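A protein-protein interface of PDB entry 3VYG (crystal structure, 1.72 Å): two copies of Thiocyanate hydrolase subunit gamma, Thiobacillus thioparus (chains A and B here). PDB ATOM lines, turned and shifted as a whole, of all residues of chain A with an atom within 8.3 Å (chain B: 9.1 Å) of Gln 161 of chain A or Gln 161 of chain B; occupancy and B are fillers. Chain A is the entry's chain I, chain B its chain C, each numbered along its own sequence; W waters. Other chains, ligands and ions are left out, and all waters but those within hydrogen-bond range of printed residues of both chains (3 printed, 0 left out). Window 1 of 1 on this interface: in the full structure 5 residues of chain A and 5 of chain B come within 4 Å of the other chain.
Arg 154 of chain A touches Gln 161 of chain B, but with the chains exchanged Gln 161 of chain A does not touch Arg 154 of chain B (7.2 Å).
Gln 161 of chain A touches Ala 164 of chain B, but with the chains exchanged Ala 164 of chain A does not touch Gln 161 of chain B (6.4 Å).
Gln 161 of chain A touches Glu 165 of chain B, and with the chains exchanged Glu 165 of chain A touches Gln 161 of chain B.
Gln 169 of chain B touches its own counterpart, Gln 169 of chain A.
The guanidinium group (NH1) of Arg 154 of chain B is in salt-bridge range of the side-chain carboxylate (OE2) of Glu 165 of chain B (2.8 Å).
The side-chain amide oxygen of Gln 161 of chain A sits close to the backbone carbonyl oxygen of Trp 158 of chain A (3.3 Å).
NH1 of Arg 154 of chain A is in salt-bridge range of OE2 of Glu 165 of chain A (2.8 Å).
Printed residues of chain B within 4 Å of Arg 154 of chain A: Gln 161 (3.7 Å).
Gln 161 of chain A touches three residues of chain B.
No residue of chain B comes within 4 Å of Val 162 of chain A.
Arg 154 of chain B touches none of the printed residues of chain A.
Trp 158 of chain B touches none of the printed residues of chain A.
Of the printed residues of chain A, Gln 161 of chain B touches Arg 154, Gln 161 and Glu 165.
Ala 164 of chain B touches just one residue of chain A: Gln 161 (3.8 Å).
Of the printed residues of chain A, Glu 165 of chain B touches Gln 161.
The nearest printed residue of chain A that does not touch Gln 161 of chain B is Trp 158 of chain A (5.6 Å).
Among the printed residues, merely in contact across the chains: Gln 161 of chain A with Glu 165 of chain B (3.4 Å), Gln 169 of chain A with Gln 169 of chain B (3.6 Å), Arg 154 of chain A with Gln 161 of chain B (3.7 Å), Gln 161 of chain A with Ala 164 of chain B (3.8 Å), Gln 161 of chain A with Gln 161 of chain B (3.9 Å) and Glu 165 of chain A with Gln 161 of chain B (3.99 Å).
Water W1 lies within hydrogen-bond range of the side-chain amide nitrogen of Gln 169 of chain B (2.8 Å) and the guanidinium group of Arg 160 of chain A (3.1 Å).
Water W3 bridges the side-chain amide nitrogen of Gln 169 of chain A (2.8 Å) and the guanidinium group of Arg 160 of chain B (3.0 Å).
Water W2 bridges NH1 of Arg 154 of chain A (3.0 Å) and NE2 of Gln 161 of chain B (3.1 Å).
Printed residues of chain A that touch a printed residue of chain B: Arg 154, Gln 161, Glu 165 and Gln 169.
Printed residues of chain B that touch a printed residue of chain A: Gln 161, Ala 164, Glu 165 and Gln 169.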
ATOM      1  N   ARG A 154      -6.529 -22.300 -13.794  1.00  0.00           N
ATOM      2  CA  ARG A 154      -7.738 -22.311 -12.969  1.00  0.00           C
ATOM      3  C   ARG A 154      -7.494 -22.565 -11.508  1.00  0.00           C
ATOM      4  O   ARG A 154      -8.213 -22.024 -10.723  1.00  0.00           O
ATOM      5  CB  ARG A 154      -8.715 -23.351 -13.471  1.00  0.00           C
ATOM      6  CG  ARG A 154      -9.329 -23.080 -14.970  1.00  0.00           C
ATOM      7  CD  ARG A 154     -10.668 -23.865 -15.148  1.00  0.00           C
ATOM      8  NE  ARG A 154     -10.398 -25.281 -15.097  1.00  0.00           N
ATOM      9  CZ  ARG A 154     -11.227 -26.274 -14.742  1.00  0.00           C
ATOM     10  NH1 ARG A 154     -12.504 -26.027 -14.457  1.00  0.00           N
ATOM     11  NH2 ARG A 154     -10.775 -27.532 -14.649  1.00  0.00           N
ATOM     12  N   LEU A 155      -6.559 -23.475 -11.184  1.00  0.00           N
ATOM     13  CA  LEU A 155      -6.378 -23.778  -9.774  1.00  0.00           C
ATOM     14  C   LEU A 155      -6.125 -22.609  -8.874  1.00  0.00           C
ATOM     15  O   LEU A 155      -6.715 -22.570  -7.754  1.00  0.00           O
ATOM     16  CB  LEU A 155      -5.206 -24.769  -9.588  1.00  0.00           C
ATOM     17  CG  LEU A 155      -5.034 -25.319  -8.113  1.00  0.00           C
ATOM     18  CD1 LEU A 155      -6.083 -26.490  -7.932  1.00  0.00           C
ATOM     19  CD2 LEU A 155      -3.669 -25.801  -7.829  1.00  0.00           C
ATOM     20  N   VAL A 156      -5.244 -21.644  -9.228  1.00  0.00           N
ATOM     21  CA  VAL A 156      -5.000 -20.501  -8.401  1.00  0.00           C
ATOM     22  C   VAL A 156      -6.187 -19.669  -8.040  1.00  0.00           C
ATOM     23  O   VAL A 156      -6.239 -19.033  -7.025  1.00  0.00           O
ATOM     24  CB  VAL A 156      -3.870 -19.529  -8.859  1.00  0.00           C
ATOM     25  CG1 VAL A 156      -2.594 -20.159  -8.741  1.00  0.00           C
ATOM     26  CG2 VAL A 156      -4.141 -19.066 -10.383  1.00  0.00           C
ATOM     27  N   ARG A 157      -7.178 -19.652  -8.936  1.00  0.00           N
ATOM     28  CA  ARG A 157      -8.238 -18.690  -8.785  1.00  0.00           C
ATOM     29  C   ARG A 157      -9.599 -19.424  -8.382  1.00  0.00           C
ATOM     30  O   ARG A 157     -10.429 -18.765  -7.684  1.00  0.00           O
ATOM     31  CB  ARG A 157      -8.473 -18.045 -10.219  1.00  0.00           C
ATOM     32  CG  ARG A 157      -9.560 -16.962 -10.104  1.00  0.00           C
ATOM     33  CD  ARG A 157      -9.468 -16.070 -11.366  1.00  0.00           C
ATOM     34  NE  ARG A 157     -10.360 -14.916 -11.163  1.00  0.00           N
ATOM     35  CZ  ARG A 157     -10.229 -13.758 -11.833  1.00  0.00           C
ATOM     36  NH1 ARG A 157      -9.299 -13.643 -12.811  1.00  0.00           N
ATOM     37  NH2 ARG A 157     -10.972 -12.710 -11.496  1.00  0.00           N
ATOM     38  N   TRP A 158      -9.811 -20.664  -8.801  1.00  0.00           N
ATOM     39  CA  TRP A 158     -11.005 -21.484  -8.406  1.00  0.00           C
ATOM     40  C   TRP A 158     -10.590 -22.815  -7.831  1.00  0.00           C
ATOM     41  O   TRP A 158     -10.892 -23.844  -8.372  1.00  0.00           O
ATOM     42  CB  TRP A 158     -11.881 -21.738  -9.657  1.00  0.00           C
ATOM     43  CG  TRP A 158     -12.354 -20.409 -10.311  1.00  0.00           C
ATOM     44  CD1 TRP A 158     -13.382 -19.579  -9.901  1.00  0.00           C
ATOM     45  CD2 TRP A 158     -11.784 -19.779 -11.496  1.00  0.00           C
ATOM     46  NE1 TRP A 158     -13.444 -18.466 -10.722  1.00  0.00           N
ATOM     47  CE2 TRP A 158     -12.488 -18.593 -11.713  1.00  0.00           C
ATOM     48  CE3 TRP A 158     -10.712 -20.131 -12.393  1.00  0.00           C
ATOM     49  CZ2 TRP A 158     -12.208 -17.707 -12.848  1.00  0.00           C
ATOM     50  CZ3 TRP A 158     -10.375 -19.210 -13.512  1.00  0.00           C
ATOM     51  CH2 TRP A 158     -11.115 -18.016 -13.682  1.00  0.00           C
ATOM     52  N   PRO A 159      -9.751 -22.783  -6.768  1.00  0.00           N
ATOM     53  CA  PRO A 159      -9.220 -24.091  -6.313  1.00  0.00           C
ATOM     54  C   PRO A 159     -10.283 -25.034  -5.794  1.00  0.00           C
ATOM     55  O   PRO A 159     -10.148 -26.246  -6.026  1.00  0.00           O
ATOM     56  CB  PRO A 159      -8.248 -23.680  -5.165  1.00  0.00           C
ATOM     57  CG  PRO A 159      -8.729 -22.355  -4.677  1.00  0.00           C
ATOM     58  CD  PRO A 159      -9.153 -21.659  -6.062  1.00  0.00           C
ATOM     59  N   ARG A 160     -11.305 -24.522  -5.107  1.00  0.00           N
ATOM     60  CA  ARG A 160     -12.367 -25.451  -4.588  1.00  0.00           C
ATOM     61  C   ARG A 160     -13.135 -26.087  -5.733  1.00  0.00           C
ATOM     62  O   ARG A 160     -13.431 -27.250  -5.706  1.00  0.00           O
ATOM     63  CB  ARG A 160     -13.308 -24.646  -3.718  1.00  0.00           C
ATOM     64  CG  ARG A 160     -12.546 -24.313  -2.374  1.00  0.00           C
ATOM     65  CD  ARG A 160     -13.425 -23.938  -1.372  1.00  0.00           C
ATOM     66  NE  ARG A 160     -12.716 -23.515  -0.158  1.00  0.00           N
ATOM     67  CZ  ARG A 160     -12.814 -24.159   1.009  1.00  0.00           C
ATOM     68  NH1 ARG A 160     -13.488 -25.272   1.109  1.00  0.00           N
ATOM     69  NH2 ARG A 160     -12.260 -23.596   2.082  1.00  0.00           N
ATOM     70  N   GLN A 161     -13.321 -25.313  -6.816  1.00  0.00           N
ATOM     71  CA  GLN A 161     -13.936 -25.886  -8.057  1.00  0.00           C
ATOM     72  C   GLN A 161     -13.126 -26.908  -8.752  1.00  0.00           C
ATOM     73  O   GLN A 161     -13.686 -27.937  -9.123  1.00  0.00           O
ATOM     74  CB  GLN A 161     -14.394 -24.723  -9.016  1.00  0.00           C
ATOM     75  CG  GLN A 161     -15.402 -23.648  -8.262  1.00  0.00           C
ATOM     76  CD  GLN A 161     -14.755 -22.506  -7.523  1.00  0.00           C
ATOM     77  OE1 GLN A 161     -13.629 -22.625  -7.102  1.00  0.00           O
ATOM     78  NE2 GLN A 161     -15.449 -21.390  -7.357  1.00  0.00           N
ATOM     79  N   VAL A 162     -11.777 -26.723  -8.823  1.00  0.00           N
ATOM     80  CA  VAL A 162     -10.969 -27.674  -9.488  1.00  0.00           C
ATOM     81  C   VAL A 162     -10.826 -28.921  -8.585  1.00  0.00           C
ATOM     82  O   VAL A 162     -10.976 -30.044  -9.059  1.00  0.00           O
ATOM     83  CB  VAL A 162      -9.562 -27.038  -9.755  1.00  0.00           C
ATOM     84  CG1 VAL A 162      -8.628 -28.118 -10.317  1.00  0.00           C
ATOM     85  CG2 VAL A 162      -9.743 -25.822 -10.844  1.00  0.00           C
ATOM     86  N   LEU A 163     -10.615 -28.705  -7.278  1.00  0.00           N
ATOM     87  CA  LEU A 163     -10.499 -29.859  -6.373  1.00  0.00           C
ATOM     88  C   LEU A 163     -11.792 -30.690  -6.427  1.00  0.00           C
ATOM     89  O   LEU A 163     -11.748 -31.940  -6.345  1.00  0.00           O
ATOM     90  CB  LEU A 163     -10.303 -29.383  -4.950  1.00  0.00           C
ATOM     91  CG  LEU A 163      -8.887 -28.791  -4.744  1.00  0.00           C
ATOM     92  CD1 LEU A 163      -8.779 -28.305  -3.256  1.00  0.00           C
ATOM     93  CD2 LEU A 163      -7.825 -29.889  -5.006  1.00  0.00           C
ATOM     94  N   ALA A 164     -12.943 -30.038  -6.515  1.00  0.00           N
ATOM     95  CA  ALA A 164     -14.172 -30.822  -6.545  1.00  0.00           C
ATOM     96  C   ALA A 164     -14.238 -31.748  -7.760  1.00  0.00           C
ATOM     97  O   ALA A 164     -14.746 -32.897  -7.645  1.00  0.00           O
ATOM     98  CB  ALA A 164     -15.399 -29.868  -6.403  1.00  0.00           C
ATOM     99  N   GLU A 165     -13.658 -31.337  -8.895  1.00  0.00           N
ATOM    100  CA  GLU A 165     -13.562 -32.144 -10.088  1.00  0.00           C
ATOM    101  C   GLU A 165     -12.679 -33.382  -9.873  1.00  0.00           C
ATOM    102  O   GLU A 165     -12.829 -34.425 -10.571  1.00  0.00           O
ATOM    103  CB  GLU A 165     -12.959 -31.347 -11.253  1.00  0.00           C
ATOM    104  CG  GLU A 165     -13.710 -30.063 -11.646  1.00  0.00           C
ATOM    105  CD  GLU A 165     -13.094 -29.286 -12.869  1.00  0.00           C
ATOM    106  OE1 GLU A 165     -12.018 -29.718 -13.449  1.00  0.00           O
ATOM    107  OE2 GLU A 165     -13.687 -28.213 -13.232  1.00  0.00           O
ATOM    108  N   PHE A 166     -11.692 -33.246  -8.981  1.00  0.00           N
ATOM    109  CA  PHE A 166     -10.811 -34.335  -8.628  1.00  0.00           C
ATOM    110  C   PHE A 166     -11.443 -35.198  -7.562  1.00  0.00           C
ATOM    111  O   PHE A 166     -10.860 -36.197  -7.176  1.00  0.00           O
ATOM    112  CB  PHE A 166      -9.469 -33.777  -8.080  1.00  0.00           C
ATOM    113  CG  PHE A 166      -8.499 -33.383  -9.176  1.00  0.00           C
ATOM    114  CD1 PHE A 166      -8.355 -32.060  -9.578  1.00  0.00           C
ATOM    115  CD2 PHE A 166      -7.745 -34.373  -9.819  1.00  0.00           C
ATOM    116  CE1 PHE A 166      -7.422 -31.725 -10.612  1.00  0.00           C
ATOM    117  CE2 PHE A 166      -6.821 -34.061 -10.810  1.00  0.00           C
ATOM    118  CZ  PHE A 166      -6.648 -32.763 -11.222  1.00  0.00           C
ATOM    119  N   GLY A 167     -12.618 -34.817  -7.097  1.00  0.00           N
ATOM    120  CA  GLY A 167     -13.392 -35.565  -6.096  1.00  0.00           C
ATOM    121  C   GLY A 167     -13.079 -35.197  -4.671  1.00  0.00           C
ATOM    122  O   GLY A 167     -13.330 -35.984  -3.760  1.00  0.00           O
ATOM    123  N   LEU A 168     -12.545 -34.001  -4.458  1.00  0.00           N
ATOM    124  CA  LEU A 168     -12.231 -33.518  -3.106  1.00  0.00           C
ATOM    125  C   LEU A 168     -12.969 -32.224  -2.724  1.00  0.00           C
ATOM    126  O   LEU A 168     -12.799 -31.201  -3.365  1.00  0.00           O
ATOM    127  CB  LEU A 168     -10.695 -33.271  -3.002  1.00  0.00           C
ATOM    128  CG  LEU A 168     -10.206 -32.788  -1.642  1.00  0.00           C
ATOM    129  CD1 LEU A 168     -10.571 -33.731  -0.466  1.00  0.00           C
ATOM    130  CD2 LEU A 168      -8.659 -32.686  -1.825  1.00  0.00           C
ATOM    131  N   GLN A 169     -13.670 -32.222  -1.581  1.00  0.00           N
ATOM    132  CA  GLN A 169     -14.272 -30.992  -1.036  1.00  0.00           C
ATOM    133  C   GLN A 169     -13.886 -30.935   0.453  1.00  0.00           C
ATOM    134  O   GLN A 169     -13.757 -32.019   1.151  1.00  0.00           O
ATOM    135  CB  GLN A 169     -15.805 -31.087  -1.106  1.00  0.00           C
ATOM    136  CG  GLN A 169     -16.390 -30.767  -2.441  1.00  0.00           C
ATOM    137  CD  GLN A 169     -17.945 -30.693  -2.415  1.00  0.00           C
ATOM    138  OE1 GLN A 169     -18.597 -31.315  -1.563  1.00  0.00           O
ATOM    139  NE2 GLN A 169     -18.538 -29.979  -3.416  1.00  0.00           N
ATOM    140  N   ILE A 176      -8.125 -23.453   2.428  1.00  0.00           N
ATOM    141  CA  ILE A 176      -7.426 -24.081   1.343  1.00  0.00           C
ATOM    142  C   ILE A 176      -6.318 -23.139   0.898  1.00  0.00           C
ATOM    143  O   ILE A 176      -6.550 -21.919   0.633  1.00  0.00           O
ATOM    144  CB  ILE A 176      -8.376 -24.298   0.074  1.00  0.00           C
ATOM    145  CG1 ILE A 176      -9.512 -25.233   0.458  1.00  0.00           C
ATOM    146  CG2 ILE A 176      -7.484 -24.732  -1.117  1.00  0.00           C
ATOM    147  CD1 ILE A 176      -9.123 -26.655   0.698  1.00  0.00           C
ATOM    148  N   ASN B 150     -23.999 -17.451 -20.025  1.00  0.00           N
ATOM    149  CA  ASN B 150     -23.042 -18.231 -19.174  1.00  0.00           C
ATOM    150  C   ASN B 150     -23.765 -19.111 -18.140  1.00  0.00           C
ATOM    151  O   ASN B 150     -23.589 -20.311 -18.123  1.00  0.00           O
ATOM    152  CB  ASN B 150     -22.104 -17.271 -18.520  1.00  0.00           C
ATOM    153  CG  ASN B 150     -21.059 -17.977 -17.745  1.00  0.00           C
ATOM    154  OD1 ASN B 150     -21.341 -18.532 -16.701  1.00  0.00           O
ATOM    155  ND2 ASN B 150     -19.805 -18.018 -18.298  1.00  0.00           N
ATOM    156  N   ARG B 154     -24.060 -23.336 -18.299  1.00  0.00           N
ATOM    157  CA  ARG B 154     -23.220 -24.071 -17.319  1.00  0.00           C
ATOM    158  C   ARG B 154     -23.976 -24.723 -16.160  1.00  0.00           C
ATOM    159  O   ARG B 154     -23.632 -25.832 -15.799  1.00  0.00           O
ATOM    160  CB  ARG B 154     -22.181 -23.148 -16.707  1.00  0.00           C
ATOM    161  CG  ARG B 154     -21.136 -22.739 -17.733  1.00  0.00           C
ATOM    162  CD  ARG B 154     -19.884 -22.227 -16.933  1.00  0.00           C
ATOM    163  NE  ARG B 154     -20.136 -21.141 -16.059  1.00  0.00           N
ATOM    164  CZ  ARG B 154     -19.532 -20.835 -14.881  1.00  0.00           C
ATOM    165  NH1 ARG B 154     -18.489 -21.619 -14.448  1.00  0.00           N
ATOM    166  NH2 ARG B 154     -19.926 -19.837 -14.105  1.00  0.00           N
ATOM    167  N   LEU B 155     -25.013 -24.116 -15.658  1.00  0.00           N
ATOM    168  CA  LEU B 155     -25.657 -24.735 -14.482  1.00  0.00           C
ATOM    169  C   LEU B 155     -26.167 -26.134 -14.712  1.00  0.00           C
ATOM    170  O   LEU B 155     -26.035 -26.987 -13.806  1.00  0.00           O
ATOM    171  CB  LEU B 155     -26.829 -23.839 -14.008  1.00  0.00           C
ATOM    172  CG  LEU B 155     -27.433 -24.272 -12.659  1.00  0.00           C
ATOM    173  CD1 LEU B 155     -26.476 -23.878 -11.466  1.00  0.00           C
ATOM    174  CD2 LEU B 155     -28.874 -23.693 -12.404  1.00  0.00           C
ATOM    175  N   ARG B 157     -25.049 -28.485 -16.457  1.00  0.00           N
ATOM    176  CA  ARG B 157     -24.017 -29.471 -16.677  1.00  0.00           C
ATOM    177  C   ARG B 157     -22.950 -29.507 -15.524  1.00  0.00           C
ATOM    178  O   ARG B 157     -22.376 -30.605 -15.260  1.00  0.00           O
ATOM    179  CB  ARG B 157     -23.346 -29.209 -18.030  1.00  0.00           C
ATOM    180  CG  ARG B 157     -22.274 -30.304 -18.411  1.00  0.00           C
ATOM    181  CD  ARG B 157     -21.849 -30.151 -19.870  1.00  0.00           C
ATOM    182  NE  ARG B 157     -20.962 -31.213 -20.325  1.00  0.00           N
ATOM    183  CZ  ARG B 157     -20.883 -31.632 -21.587  1.00  0.00           C
ATOM    184  NH1 ARG B 157     -21.492 -30.982 -22.620  1.00  0.00           N
ATOM    185  NH2 ARG B 157     -20.143 -32.726 -21.822  1.00  0.00           N
ATOM    186  N   TRP B 158     -22.622 -28.387 -14.975  1.00  0.00           N
ATOM    187  CA  TRP B 158     -21.647 -28.312 -13.869  1.00  0.00           C
ATOM    188  C   TRP B 158     -22.253 -27.542 -12.741  1.00  0.00           C
ATOM    189  O   TRP B 158     -21.688 -26.553 -12.311  1.00  0.00           O
ATOM    190  CB  TRP B 158     -20.388 -27.563 -14.384  1.00  0.00           C
ATOM    191  CG  TRP B 158     -19.724 -28.207 -15.618  1.00  0.00           C
ATOM    192  CD1 TRP B 158     -18.799 -29.246 -15.642  1.00  0.00           C
ATOM    193  CD2 TRP B 158     -19.856 -27.782 -16.962  1.00  0.00           C
ATOM    194  NE1 TRP B 158     -18.432 -29.564 -16.934  1.00  0.00           N
ATOM    195  CE2 TRP B 158     -19.026 -28.645 -17.759  1.00  0.00           C
ATOM    196  CE3 TRP B 158     -20.626 -26.768 -17.581  1.00  0.00           C
ATOM    197  CZ2 TRP B 158     -18.920 -28.518 -19.102  1.00  0.00           C
ATOM    198  CZ3 TRP B 158     -20.523 -26.635 -18.947  1.00  0.00           C
ATOM    199  CH2 TRP B 158     -19.684 -27.509 -19.694  1.00  0.00           C
ATOM    200  N   PRO B 159     -23.370 -28.000 -12.177  1.00  0.00           N
ATOM    201  CA  PRO B 159     -23.981 -27.205 -11.148  1.00  0.00           C
ATOM    202  C   PRO B 159     -23.121 -27.027  -9.917  1.00  0.00           C
ATOM    203  O   PRO B 159     -23.188 -26.005  -9.252  1.00  0.00           O
ATOM    204  CB  PRO B 159     -25.288 -28.004 -10.770  1.00  0.00           C
ATOM    205  CG  PRO B 159     -25.038 -29.442 -11.273  1.00  0.00           C
ATOM    206  CD  PRO B 159     -24.125 -29.218 -12.565  1.00  0.00           C
ATOM    207  N   ARG B 160     -22.343 -28.089  -9.561  1.00  0.00           N
ATOM    208  CA  ARG B 160     -21.624 -27.893  -8.262  1.00  0.00           C
ATOM    209  C   ARG B 160     -20.485 -26.894  -8.501  1.00  0.00           C
ATOM    210  O   ARG B 160     -20.121 -26.179  -7.572  1.00  0.00           O
ATOM    211  CB  ARG B 160     -21.069 -29.244  -7.832  1.00  0.00           C
ATOM    212  CG  ARG B 160     -22.114 -29.909  -6.985  1.00  0.00           C
ATOM    213  CD  ARG B 160     -21.806 -31.259  -6.857  1.00  0.00           C
ATOM    214  NE  ARG B 160     -22.874 -32.092  -6.289  1.00  0.00           N
ATOM    215  CZ  ARG B 160     -23.072 -32.409  -5.009  1.00  0.00           C
ATOM    216  NH1 ARG B 160     -22.499 -31.750  -3.999  1.00  0.00           N
ATOM    217  NH2 ARG B 160     -24.014 -33.316  -4.753  1.00  0.00           N
ATOM    218  N   GLN B 161     -19.950 -26.825  -9.746  1.00  0.00           N
ATOM    219  CA  GLN B 161     -18.966 -25.728 -10.036  1.00  0.00           C
ATOM    220  C   GLN B 161     -19.587 -24.331  -9.942  1.00  0.00           C
ATOM    221  O   GLN B 161     -19.132 -23.423  -9.245  1.00  0.00           O
ATOM    222  CB  GLN B 161     -18.335 -25.935 -11.398  1.00  0.00           C
ATOM    223  CG  GLN B 161     -17.394 -24.772 -11.715  1.00  0.00           C
ATOM    224  CD  GLN B 161     -16.578 -25.008 -12.960  1.00  0.00           C
ATOM    225  OE1 GLN B 161     -16.911 -25.922 -13.768  1.00  0.00           O
ATOM    226  NE2 GLN B 161     -15.468 -24.228 -13.099  1.00  0.00           N
ATOM    227  N   VAL B 162     -20.779 -24.177 -10.543  1.00  0.00           N
ATOM    228  CA  VAL B 162     -21.429 -22.865 -10.472  1.00  0.00           C
ATOM    229  C   VAL B 162     -21.853 -22.478  -9.078  1.00  0.00           C
ATOM    230  O   VAL B 162     -21.646 -21.356  -8.638  1.00  0.00           O
ATOM    231  CB  VAL B 162     -22.676 -22.844 -11.389  1.00  0.00           C
ATOM    232  CG1 VAL B 162     -23.489 -21.490 -11.253  1.00  0.00           C
ATOM    233  CG2 VAL B 162     -22.273 -23.087 -12.854  1.00  0.00           C
ATOM    234  N   LEU B 163     -22.465 -23.423  -8.338  1.00  0.00           N
ATOM    235  CA  LEU B 163     -22.863 -23.119  -6.982  1.00  0.00           C
ATOM    236  C   LEU B 163     -21.667 -22.736  -6.086  1.00  0.00           C
ATOM    237  O   LEU B 163     -21.781 -21.871  -5.269  1.00  0.00           O
ATOM    238  CB  LEU B 163     -23.624 -24.319  -6.357  1.00  0.00           C
ATOM    239  CG  LEU B 163     -25.029 -24.571  -6.996  1.00  0.00           C
ATOM    240  CD1 LEU B 163     -25.581 -25.899  -6.382  1.00  0.00           C
ATOM    241  CD2 LEU B 163     -25.959 -23.384  -6.720  1.00  0.00           C
ATOM    242  N   ALA B 164     -20.554 -23.405  -6.332  1.00  0.00           N
ATOM    243  CA  ALA B 164     -19.363 -23.079  -5.517  1.00  0.00           C
ATOM    244  C   ALA B 164     -18.850 -21.686  -5.801  1.00  0.00           C
ATOM    245  O   ALA B 164     -18.327 -20.979  -4.912  1.00  0.00           O
ATOM    246  CB  ALA B 164     -18.308 -24.175  -5.757  1.00  0.00           C
ATOM    247  N   GLU B 165     -19.072 -21.196  -7.051  1.00  0.00           N
ATOM    248  CA  GLU B 165     -18.782 -19.769  -7.340  1.00  0.00           C
ATOM    249  C   GLU B 165     -19.673 -18.826  -6.602  1.00  0.00           C
ATOM    250  O   GLU B 165     -19.307 -17.683  -6.229  1.00  0.00           O
ATOM    251  CB  GLU B 165     -18.796 -19.500  -8.840  1.00  0.00           C
ATOM    252  CG  GLU B 165     -17.797 -20.332  -9.603  1.00  0.00           C
ATOM    253  CD  GLU B 165     -18.014 -20.277 -11.149  1.00  0.00           C
ATOM    254  OE1 GLU B 165     -18.800 -19.403 -11.542  1.00  0.00           O
ATOM    255  OE2 GLU B 165     -17.457 -21.104 -11.904  1.00  0.00           O
ATOM    256  N   PHE B 166     -20.851 -19.304  -6.225  1.00  0.00           N
ATOM    257  CA  PHE B 166     -21.697 -18.506  -5.379  1.00  0.00           C
ATOM    258  C   PHE B 166     -21.480 -18.748  -3.855  1.00  0.00           C
ATOM    259  O   PHE B 166     -22.142 -18.134  -3.038  1.00  0.00           O
ATOM    260  CB  PHE B 166     -23.186 -18.886  -5.651  1.00  0.00           C
ATOM    261  CG  PHE B 166     -23.757 -18.287  -6.931  1.00  0.00           C
ATOM    262  CD1 PHE B 166     -23.709 -18.969  -8.119  1.00  0.00           C
ATOM    263  CD2 PHE B 166     -24.356 -17.010  -6.890  1.00  0.00           C
ATOM    264  CE1 PHE B 166     -24.300 -18.394  -9.283  1.00  0.00           C
ATOM    265  CE2 PHE B 166     -24.943 -16.411  -8.060  1.00  0.00           C
ATOM    266  CZ  PHE B 166     -24.894 -17.098  -9.235  1.00  0.00           C
ATOM    267  N   GLY B 167     -20.495 -19.572  -3.512  1.00  0.00           N
ATOM    268  CA  GLY B 167     -20.207 -19.835  -2.129  1.00  0.00           C
ATOM    269  C   GLY B 167     -20.996 -20.977  -1.549  1.00  0.00           C
ATOM    270  O   GLY B 167     -20.999 -21.161  -0.327  1.00  0.00           O
ATOM    271  N   LEU B 168     -21.658 -21.758  -2.381  1.00  0.00           N
ATOM    272  CA  LEU B 168     -22.456 -22.862  -1.850  1.00  0.00           C
ATOM    273  C   LEU B 168     -21.838 -24.175  -2.271  1.00  0.00           C
ATOM    274  O   LEU B 168     -21.782 -24.561  -3.459  1.00  0.00           O
ATOM    275  CB  LEU B 168     -23.914 -22.780  -2.401  1.00  0.00           C
ATOM    276  CG  LEU B 168     -24.788 -23.949  -1.964  1.00  0.00           C
ATOM    277  CD1 LEU B 168     -24.851 -23.959  -0.392  1.00  0.00           C
ATOM    278  CD2 LEU B 168     -26.192 -23.577  -2.452  1.00  0.00           C
ATOM    279  N   GLN B 169     -21.515 -24.982  -1.249  1.00  0.00           N
ATOM    280  CA  GLN B 169     -21.120 -26.294  -1.507  1.00  0.00           C
ATOM    281  C   GLN B 169     -21.961 -27.240  -0.580  1.00  0.00           C
ATOM    282  O   GLN B 169     -22.414 -26.768   0.497  1.00  0.00           O
ATOM    283  CB  GLN B 169     -19.613 -26.314  -1.205  1.00  0.00           C
ATOM    284  CG  GLN B 169     -18.982 -27.524  -0.847  1.00  0.00           C
ATOM    285  CD  GLN B 169     -17.516 -27.100  -0.406  1.00  0.00           C
ATOM    286  OE1 GLN B 169     -17.238 -26.880   0.827  1.00  0.00           O
ATOM    287  NE2 GLN B 169     -16.685 -26.817  -1.419  1.00  0.00           N
ATOM    288  N   ILE B 176     -28.103 -32.799  -5.720  1.00  0.00           N
ATOM    289  CA  ILE B 176     -28.371 -31.471  -6.256  1.00  0.00           C
ATOM    290  C   ILE B 176     -29.255 -31.695  -7.498  1.00  0.00           C
ATOM    291  O   ILE B 176     -28.985 -32.527  -8.316  1.00  0.00           O
ATOM    292  CB  ILE B 176     -27.082 -30.746  -6.712  1.00  0.00           C
ATOM    293  CG1 ILE B 176     -26.198 -30.554  -5.543  1.00  0.00           C
ATOM    294  CG2 ILE B 176     -27.474 -29.390  -7.303  1.00  0.00           C
ATOM    295  CD1 ILE B 176     -26.713 -29.681  -4.602  1.00  0.00           C
HETATM  296  O   HOH W   1     -14.049 -27.470  -0.933  1.00  0.00           O
HETATM  297  O   HOH W   2     -14.054 -23.885 -15.783  1.00  0.00           O
HETATM  298  O   HOH W   3     -21.152 -29.057  -3.822  1.00  0.00           O
